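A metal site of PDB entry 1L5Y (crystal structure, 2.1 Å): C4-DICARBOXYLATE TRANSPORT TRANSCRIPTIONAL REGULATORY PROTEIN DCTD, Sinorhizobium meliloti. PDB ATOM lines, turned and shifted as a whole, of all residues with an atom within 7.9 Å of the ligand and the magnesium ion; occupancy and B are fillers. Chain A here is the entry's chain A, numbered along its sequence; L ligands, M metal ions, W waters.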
ATOM      1  N   ILE A   9       3.891  -9.795  23.872  1.00  0.00           N
ATOM      2  CA  ILE A   9       3.573 -10.270  22.534  1.00  0.00           C
ATOM      3  C   ILE A   9       2.092 -10.215  22.218  1.00  0.00           C
ATOM      4  O   ILE A   9       1.267 -10.766  22.949  1.00  0.00           O
ATOM      5  CB  ILE A   9       4.046 -11.755  22.314  1.00  0.00           C
ATOM      6  CG1 ILE A   9       5.527 -11.930  22.635  1.00  0.00           C
ATOM      7  CG2 ILE A   9       3.841 -12.168  20.829  1.00  0.00           C
ATOM      8  CD1 ILE A   9       5.794 -12.379  24.054  1.00  0.00           C
ATOM      9  N   ASP A  10       1.746  -9.533  21.141  1.00  0.00           N
ATOM     10  CA  ASP A  10       0.357  -9.506  20.688  1.00  0.00           C
ATOM     11  C   ASP A  10       0.375  -9.054  19.213  1.00  0.00           C
ATOM     12  O   ASP A  10       1.134  -8.148  18.854  1.00  0.00           O
ATOM     13  CB  ASP A  10      -0.504  -8.567  21.546  1.00  0.00           C
ATOM     14  CG  ASP A  10      -2.002  -8.823  21.367  1.00  0.00           C
ATOM     15  OD1 ASP A  10      -2.462  -8.751  20.209  1.00  0.00           O
ATOM     16  OD2 ASP A  10      -2.707  -9.111  22.375  1.00  0.00           O
ATOM     17  N   ASP A  11      -0.409  -9.711  18.354  1.00  0.00           N
ATOM     18  CA  ASP A  11      -0.443  -9.329  16.939  1.00  0.00           C
ATOM     19  C   ASP A  11      -1.285  -8.060  16.695  1.00  0.00           C
ATOM     20  O   ASP A  11      -1.195  -7.447  15.633  1.00  0.00           O
ATOM     21  CB  ASP A  11      -0.993 -10.492  16.095  1.00  0.00           C
ATOM     22  CG  ASP A  11      -2.399 -10.895  16.497  1.00  0.00           C
ATOM     23  OD1 ASP A  11      -2.615 -11.191  17.682  1.00  0.00           O
ATOM     24  OD2 ASP A  11      -3.276 -10.919  15.621  1.00  0.00           O
ATOM     25  N   ASP A  12      -2.076  -7.666  17.696  1.00  0.00           N
ATOM     26  CA  ASP A  12      -2.948  -6.476  17.635  1.00  0.00           C
ATOM     27  C   ASP A  12      -2.053  -5.251  17.955  1.00  0.00           C
ATOM     28  O   ASP A  12      -1.784  -4.936  19.118  1.00  0.00           O
ATOM     29  CB  ASP A  12      -4.054  -6.650  18.689  1.00  0.00           C
ATOM     30  CG  ASP A  12      -5.042  -5.495  18.719  1.00  0.00           C
ATOM     31  OD1 ASP A  12      -4.696  -4.400  18.241  1.00  0.00           O
ATOM     32  OD2 ASP A  12      -6.155  -5.696  19.247  1.00  0.00           O
ATOM     33  N   LEU A  15      -3.378  -2.551  20.536  1.00  0.00           N
ATOM     34  CA  LEU A  15      -3.431  -3.084  21.868  1.00  0.00           C
ATOM     35  C   LEU A  15      -2.006  -3.266  22.413  1.00  0.00           C
ATOM     36  O   LEU A  15      -1.731  -2.986  23.579  1.00  0.00           O
ATOM     37  CB  LEU A  15      -4.166  -4.427  21.866  1.00  0.00           C
ATOM     38  CG  LEU A  15      -4.355  -4.932  23.301  1.00  0.00           C
ATOM     39  CD1 LEU A  15      -5.065  -3.879  24.107  1.00  0.00           C
ATOM     40  CD2 LEU A  15      -5.181  -6.213  23.278  1.00  0.00           C
ATOM     41  N   ALA A  34       5.207  -8.581  17.742  1.00  0.00           N
ATOM     42  CA  ALA A  34       3.960  -9.015  17.125  1.00  0.00           C
ATOM     43  C   ALA A  34       4.080 -10.549  16.963  1.00  0.00           C
ATOM     44  O   ALA A  34       3.067 -11.253  16.885  1.00  0.00           O
ATOM     45  CB  ALA A  34       3.801  -8.363  15.730  1.00  0.00           C
ATOM     46  N   SER A  53       1.895 -12.707  26.980  1.00  0.00           N
ATOM     47  CA  SER A  53       1.521 -12.981  25.604  1.00  0.00           C
ATOM     48  C   SER A  53       0.051 -13.271  25.298  1.00  0.00           C
ATOM     49  O   SER A  53      -0.698 -13.911  26.057  1.00  0.00           O
ATOM     50  CB  SER A  53       2.384 -14.157  25.062  1.00  0.00           C
ATOM     51  OG  SER A  53       2.071 -14.436  23.705  1.00  0.00           O
ATOM     52  N   ASP A  54      -0.334 -12.751  24.153  1.00  0.00           N
ATOM     53  CA  ASP A  54      -1.644 -12.934  23.588  1.00  0.00           C
ATOM     54  C   ASP A  54      -1.672 -14.400  23.135  1.00  0.00           C
ATOM     55  O   ASP A  54      -0.626 -15.068  23.120  1.00  0.00           O
ATOM     56  CB  ASP A  54      -1.723 -11.985  22.394  1.00  0.00           C
ATOM     57  CG  ASP A  54      -2.922 -12.192  21.571  1.00  0.00           C
ATOM     58  OD1 ASP A  54      -4.051 -12.248  22.139  1.00  0.00           O
ATOM     59  OD2 ASP A  54      -2.726 -12.276  20.335  1.00  0.00           O
ATOM     60  N   ILE A  55      -2.845 -14.933  22.777  1.00  0.00           N
ATOM     61  CA  ILE A  55      -2.906 -16.320  22.330  1.00  0.00           C
ATOM     62  C   ILE A  55      -3.083 -16.514  20.823  1.00  0.00           C
ATOM     63  O   ILE A  55      -2.246 -17.199  20.176  1.00  0.00           O
ATOM     64  CB  ILE A  55      -4.022 -17.140  23.076  1.00  0.00           C
ATOM     65  CG1 ILE A  55      -3.636 -17.404  24.534  1.00  0.00           C
ATOM     66  CG2 ILE A  55      -4.216 -18.463  22.426  1.00  0.00           C
ATOM     67  CD1 ILE A  55      -4.747 -18.023  25.335  1.00  0.00           C
ATOM     68  N   ARG A  56      -4.165 -15.963  20.243  1.00  0.00           N
ATOM     69  CA  ARG A  56      -4.424 -16.160  18.805  1.00  0.00           C
ATOM     70  C   ARG A  56      -3.586 -15.212  17.965  1.00  0.00           C
ATOM     71  O   ARG A  56      -3.754 -14.008  18.022  1.00  0.00           O
ATOM     72  CB  ARG A  56      -5.919 -15.999  18.470  1.00  0.00           C
ATOM     73  CG  ARG A  56      -6.805 -17.163  19.021  1.00  0.00           C
ATOM     74  CD  ARG A  56      -6.825 -18.485  18.133  1.00  0.00           C
ATOM     75  NE  ARG A  56      -7.022 -19.627  19.028  1.00  0.00           N
ATOM     76  CZ  ARG A  56      -6.061 -20.487  19.374  1.00  0.00           C
ATOM     77  NH1 ARG A  56      -4.841 -20.345  18.862  1.00  0.00           N
ATOM     78  NH2 ARG A  56      -6.290 -21.403  20.332  1.00  0.00           N
ATOM     79  N   MET A  57      -2.703 -15.771  17.148  1.00  0.00           N
ATOM     80  CA  MET A  57      -1.825 -14.941  16.337  1.00  0.00           C
ATOM     81  C   MET A  57      -1.360 -15.675  15.091  1.00  0.00           C
ATOM     82  O   MET A  57      -1.456 -16.903  14.994  1.00  0.00           O
ATOM     83  CB  MET A  57      -0.516 -14.602  17.115  1.00  0.00           C
ATOM     84  CG  MET A  57      -0.604 -13.797  18.435  1.00  0.00           C
ATOM     85  SD  MET A  57       1.057 -13.551  19.171  1.00  0.00           S
ATOM     86  CE  MET A  57       1.190 -15.058  20.230  1.00  0.00           C
ATOM     87  N   PRO A  58      -0.850 -14.912  14.114  1.00  0.00           N
ATOM     88  CA  PRO A  58      -0.346 -15.534  12.907  1.00  0.00           C
ATOM     89  C   PRO A  58       0.920 -16.267  13.407  1.00  0.00           C
ATOM     90  O   PRO A  58       1.546 -15.850  14.405  1.00  0.00           O
ATOM     91  CB  PRO A  58       0.019 -14.346  12.021  1.00  0.00           C
ATOM     92  CG  PRO A  58      -1.032 -13.325  12.395  1.00  0.00           C
ATOM     93  CD  PRO A  58      -1.095 -13.466  13.915  1.00  0.00           C
ATOM     94  N   ASP A  61       1.215 -19.774  18.227  1.00  0.00           N
ATOM     95  CA  ASP A  61       0.262 -19.149  19.133  1.00  0.00           C
ATOM     96  C   ASP A  61       0.819 -19.036  20.565  1.00  0.00           C
ATOM     97  O   ASP A  61       1.851 -19.583  20.856  1.00  0.00           O
ATOM     98  CB  ASP A  61      -1.137 -19.839  19.058  1.00  0.00           C
ATOM     99  CG  ASP A  61      -1.313 -21.069  19.975  1.00  0.00           C
ATOM    100  OD1 ASP A  61      -0.354 -21.640  20.517  1.00  0.00           O
ATOM    101  OD2 ASP A  61      -2.487 -21.473  20.136  1.00  0.00           O
ATOM    102  N   GLY A  62       0.133 -18.292  21.425  1.00  0.00           N
ATOM    103  CA  GLY A  62       0.599 -18.057  22.780  1.00  0.00           C
ATOM    104  C   GLY A  62       0.693 -19.260  23.687  1.00  0.00           C
ATOM    105  O   GLY A  62       1.508 -19.311  24.610  1.00  0.00           O
ATOM    106  N   LEU A  80      -0.837 -15.153  30.242  1.00  0.00           N
ATOM    107  CA  LEU A  80      -1.533 -15.231  28.963  1.00  0.00           C
ATOM    108  C   LEU A  80      -2.693 -14.252  28.989  1.00  0.00           C
ATOM    109  O   LEU A  80      -3.355 -14.103  30.022  1.00  0.00           O
ATOM    110  CB  LEU A  80      -2.027 -16.657  28.717  1.00  0.00           C
ATOM    111  CG  LEU A  80      -0.877 -17.622  28.466  1.00  0.00           C
ATOM    112  CD1 LEU A  80      -1.301 -19.052  28.789  1.00  0.00           C
ATOM    113  CD2 LEU A  80      -0.378 -17.478  27.022  1.00  0.00           C
ATOM    114  N   VAL A  81      -2.907 -13.559  27.880  1.00  0.00           N
ATOM    115  CA  VAL A  81      -3.984 -12.582  27.764  1.00  0.00           C
ATOM    116  C   VAL A  81      -4.722 -12.957  26.477  1.00  0.00           C
ATOM    117  O   VAL A  81      -4.083 -13.216  25.431  1.00  0.00           O
ATOM    118  CB  VAL A  81      -3.421 -11.143  27.654  1.00  0.00           C
ATOM    119  CG1 VAL A  81      -4.550 -10.139  27.489  1.00  0.00           C
ATOM    120  CG2 VAL A  81      -2.618 -10.793  28.922  1.00  0.00           C
ATOM    121  N   THR A  82      -6.049 -13.011  26.509  1.00  0.00           N
ATOM    122  CA  THR A  82      -6.729 -13.407  25.294  1.00  0.00           C
ATOM    123  C   THR A  82      -8.171 -12.952  25.202  1.00  0.00           C
ATOM    124  O   THR A  82      -8.867 -12.840  26.215  1.00  0.00           O
ATOM    125  CB  THR A  82      -6.724 -14.935  25.137  1.00  0.00           C
ATOM    126  OG1 THR A  82      -7.311 -15.303  23.886  1.00  0.00           O
ATOM    127  CG2 THR A  82      -7.531 -15.593  26.246  1.00  0.00           C
ATOM    128  N   GLY A  83      -8.608 -12.708  23.970  1.00  0.00           N
ATOM    129  CA  GLY A  83      -9.988 -12.342  23.714  1.00  0.00           C
ATOM    130  C   GLY A  83     -10.661 -13.518  23.010  1.00  0.00           C
ATOM    131  O   GLY A  83     -11.801 -13.414  22.570  1.00  0.00           O
ATOM    132  N   HIS A  84      -9.953 -14.653  22.880  1.00  0.00           N
ATOM    133  CA  HIS A  84     -10.516 -15.815  22.210  1.00  0.00           C
ATOM    134  C   HIS A  84     -10.343 -17.081  23.071  1.00  0.00           C
ATOM    135  O   HIS A  84     -10.093 -18.169  22.552  1.00  0.00           O
ATOM    136  CB  HIS A  84      -9.833 -16.010  20.851  1.00  0.00           C
ATOM    137  CG  HIS A  84      -9.869 -14.803  19.983  1.00  0.00           C
ATOM    138  ND1 HIS A  84      -8.909 -13.814  20.062  1.00  0.00           N
ATOM    139  CD2 HIS A  84     -10.754 -14.392  19.042  1.00  0.00           C
ATOM    140  CE1 HIS A  84      -9.209 -12.854  19.196  1.00  0.00           C
ATOM    141  NE2 HIS A  84     -10.324 -13.181  18.574  1.00  0.00           N
ATOM    142  N   GLY A  85     -10.480 -16.941  24.376  1.00  0.00           N
ATOM    143  CA  GLY A  85     -10.324 -18.101  25.227  1.00  0.00           C
ATOM    144  C   GLY A  85     -11.664 -18.665  25.658  1.00  0.00           C
ATOM    145  O   GLY A  85     -12.724 -18.161  25.255  1.00  0.00           O
ATOM    146  N   MET A  89      -9.671 -24.027  28.248  1.00  0.00           N
ATOM    147  CA  MET A  89      -8.353 -23.568  27.878  1.00  0.00           C
ATOM    148  C   MET A  89      -7.678 -22.829  29.066  1.00  0.00           C
ATOM    149  O   MET A  89      -6.524 -23.067  29.349  1.00  0.00           O
ATOM    150  CB  MET A  89      -8.476 -22.634  26.692  1.00  0.00           C
ATOM    151  CG  MET A  89      -7.195 -22.088  26.138  1.00  0.00           C
ATOM    152  SD  MET A  89      -7.605 -20.729  25.018  1.00  0.00           S
ATOM    153  CE  MET A  89      -8.487 -21.535  23.737  1.00  0.00           C
ATOM    154  N   PHE A 101      -3.988 -15.975  33.618  1.00  0.00           N
ATOM    155  CA  PHE A 101      -4.709 -16.120  32.356  1.00  0.00           C
ATOM    156  C   PHE A 101      -5.800 -15.056  32.431  1.00  0.00           C
ATOM    157  O   PHE A 101      -6.725 -15.156  33.256  1.00  0.00           O
ATOM    158  CB  PHE A 101      -5.292 -17.551  32.229  1.00  0.00           C
ATOM    159  CG  PHE A 101      -5.936 -17.832  30.893  1.00  0.00           C
ATOM    160  CD1 PHE A 101      -7.195 -17.351  30.606  1.00  0.00           C
ATOM    161  CD2 PHE A 101      -5.272 -18.591  29.943  1.00  0.00           C
ATOM    162  CE1 PHE A 101      -7.811 -17.620  29.373  1.00  0.00           C
ATOM    163  CE2 PHE A 101      -5.868 -18.878  28.696  1.00  0.00           C
ATOM    164  CZ  PHE A 101      -7.136 -18.393  28.406  1.00  0.00           C
ATOM    165  N   ILE A 102      -5.681 -14.058  31.571  1.00  0.00           N
ATOM    166  CA  ILE A 102      -6.554 -12.883  31.563  1.00  0.00           C
ATOM    167  C   ILE A 102      -7.370 -12.703  30.308  1.00  0.00           C
ATOM    168  O   ILE A 102      -6.829 -12.674  29.197  1.00  0.00           O
ATOM    169  CB  ILE A 102      -5.681 -11.572  31.757  1.00  0.00           C
ATOM    170  CG1 ILE A 102      -4.836 -11.678  33.028  1.00  0.00           C
ATOM    171  CG2 ILE A 102      -6.579 -10.340  31.833  1.00  0.00           C
ATOM    172  CD1 ILE A 102      -3.930 -10.394  33.359  1.00  0.00           C
ATOM    173  N   ALA A 103      -8.665 -12.555  30.488  1.00  0.00           N
ATOM    174  CA  ALA A 103      -9.524 -12.344  29.334  1.00  0.00           C
ATOM    175  C   ALA A 103      -9.563 -10.881  28.926  1.00  0.00           C
ATOM    176  O   ALA A 103      -9.510  -9.986  29.782  1.00  0.00           O
ATOM    177  CB  ALA A 103     -10.964 -12.820  29.634  1.00  0.00           C
ATOM    178  N   LYS A 104      -9.622 -10.641  27.625  1.00  0.00           N
ATOM    179  CA  LYS A 104      -9.756  -9.279  27.087  1.00  0.00           C
ATOM    180  C   LYS A 104     -11.303  -9.182  26.990  1.00  0.00           C
ATOM    181  O   LYS A 104     -11.950 -10.150  26.631  1.00  0.00           O
ATOM    182  CB  LYS A 104      -9.174  -9.163  25.669  1.00  0.00           C
ATOM    183  CG  LYS A 104      -7.706  -9.542  25.513  1.00  0.00           C
ATOM    184  CD  LYS A 104      -7.258  -9.426  24.011  1.00  0.00           C
ATOM    185  CE  LYS A 104      -5.744  -9.596  23.870  1.00  0.00           C
ATOM    186  NZ  LYS A 104      -5.200  -9.422  22.470  1.00  0.00           N
HETATM  187 BE1  LIG L   1      -5.544 -13.015  21.419  1.00  0.00          BE
HETATM  188  F1  LIG L   1      -5.715 -12.907  19.931  1.00  0.00           F
HETATM  189  F2  LIG L   1      -5.709 -14.467  21.834  1.00  0.00           F
HETATM  190  F3  LIG L   1      -6.573 -12.106  22.088  1.00  0.00           F
HETATM  191 MG    MG M   1      -4.139 -12.137  18.746  1.00  0.00          MG
HETATM  192  O   HOH W   1      -5.571 -11.749  16.907  1.00  0.00           O
HETATM  193  O   HOH W   2      -4.628 -10.066  19.573  1.00  0.00           O
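Water W2 bridges the side-chain carboxylate (OD1) of Asp 10 and the side-chain amino group (NZ) of Lys 104.
The magnesium ion is bound by the backbone carbonyl oxygen of Arg 56 (2.0 Å), the side-chain carboxylate of Asp 11 (2.1 Å), a fluorine (F1) of the ligand (2.1 Å), the side-chain carboxylate of Asp 54 (2.1 Å), water W2 (2.3 Å) and water W1 (2.4 Å).
F1 of the ligand lies close to ND1 of His 84 (3.3 Å).
The backbone NH (N) of Arg 56 lies within hydrogen-bond range of a fluorine (F2) of the ligand, 2.7 Å away.
The backbone NH (N) of Ile 55 sits at hydrogen-bond distance from a fluorine (F2) of the ligand (3.1 Å).
NZ of Lys 104 sits at hydrogen-bond distance from F3 of the ligand.
The backbone NH (N) of Gly 83 is in hydrogen-bond range of a fluorine (F3) of the ligand.
OG1 of Thr 82 lies within hydrogen-bond range of F2 of the ligand.
OD1 of Asp 54 is bound to BE1 of the ligand, 1.8 Å away.
CG of Met 57 touches the magnesium ion, at 3.9 Å.
Four residues have an atom within 4 Å of the magnesium ion: Asp 11, Asp 54, Arg 56 and Met 57.
The nearest printed residue that does not touch the magnesium ion is Asp 10 (4.1 Å).
Hydrophobic or aromatic side chains that line the ligand: Ile 55 and His 84.
Of the 25 residues printed, 7 come within 4 Å of the ligand.
NH1 of Arg 56 is in salt-bridge range of OD2 of Asp 61 (2.9 Å).
NZ of Lys 104 is in salt-bridge range of OD2 of Asp 10 (2.5 Å).
The side-chain carboxylate of Asp 54 lies close to the side-chain amino group of Lys 104 (3.1 Å).
O of Ile 102 lies within hydrogen-bond range of N of Thr 82, at 2.8 Å.
The backbone NH (N) of Asp 54 lies within hydrogen-bond range of the backbone carbonyl oxygen (O) of Ile 9.
The backbone NH (N) of Ile 55 is in hydrogen-bond range of the backbone carbonyl oxygen (O) of Val 81, at 3.4 Å.
The backbone carbonyl oxygen (O) of Thr 82 is in hydrogen-bond range of the backbone NH (N) of Lys 104.
The backbone carbonyl oxygen of Ile 55 lies within hydrogen-bond range of the backbone NH of Gly 62.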
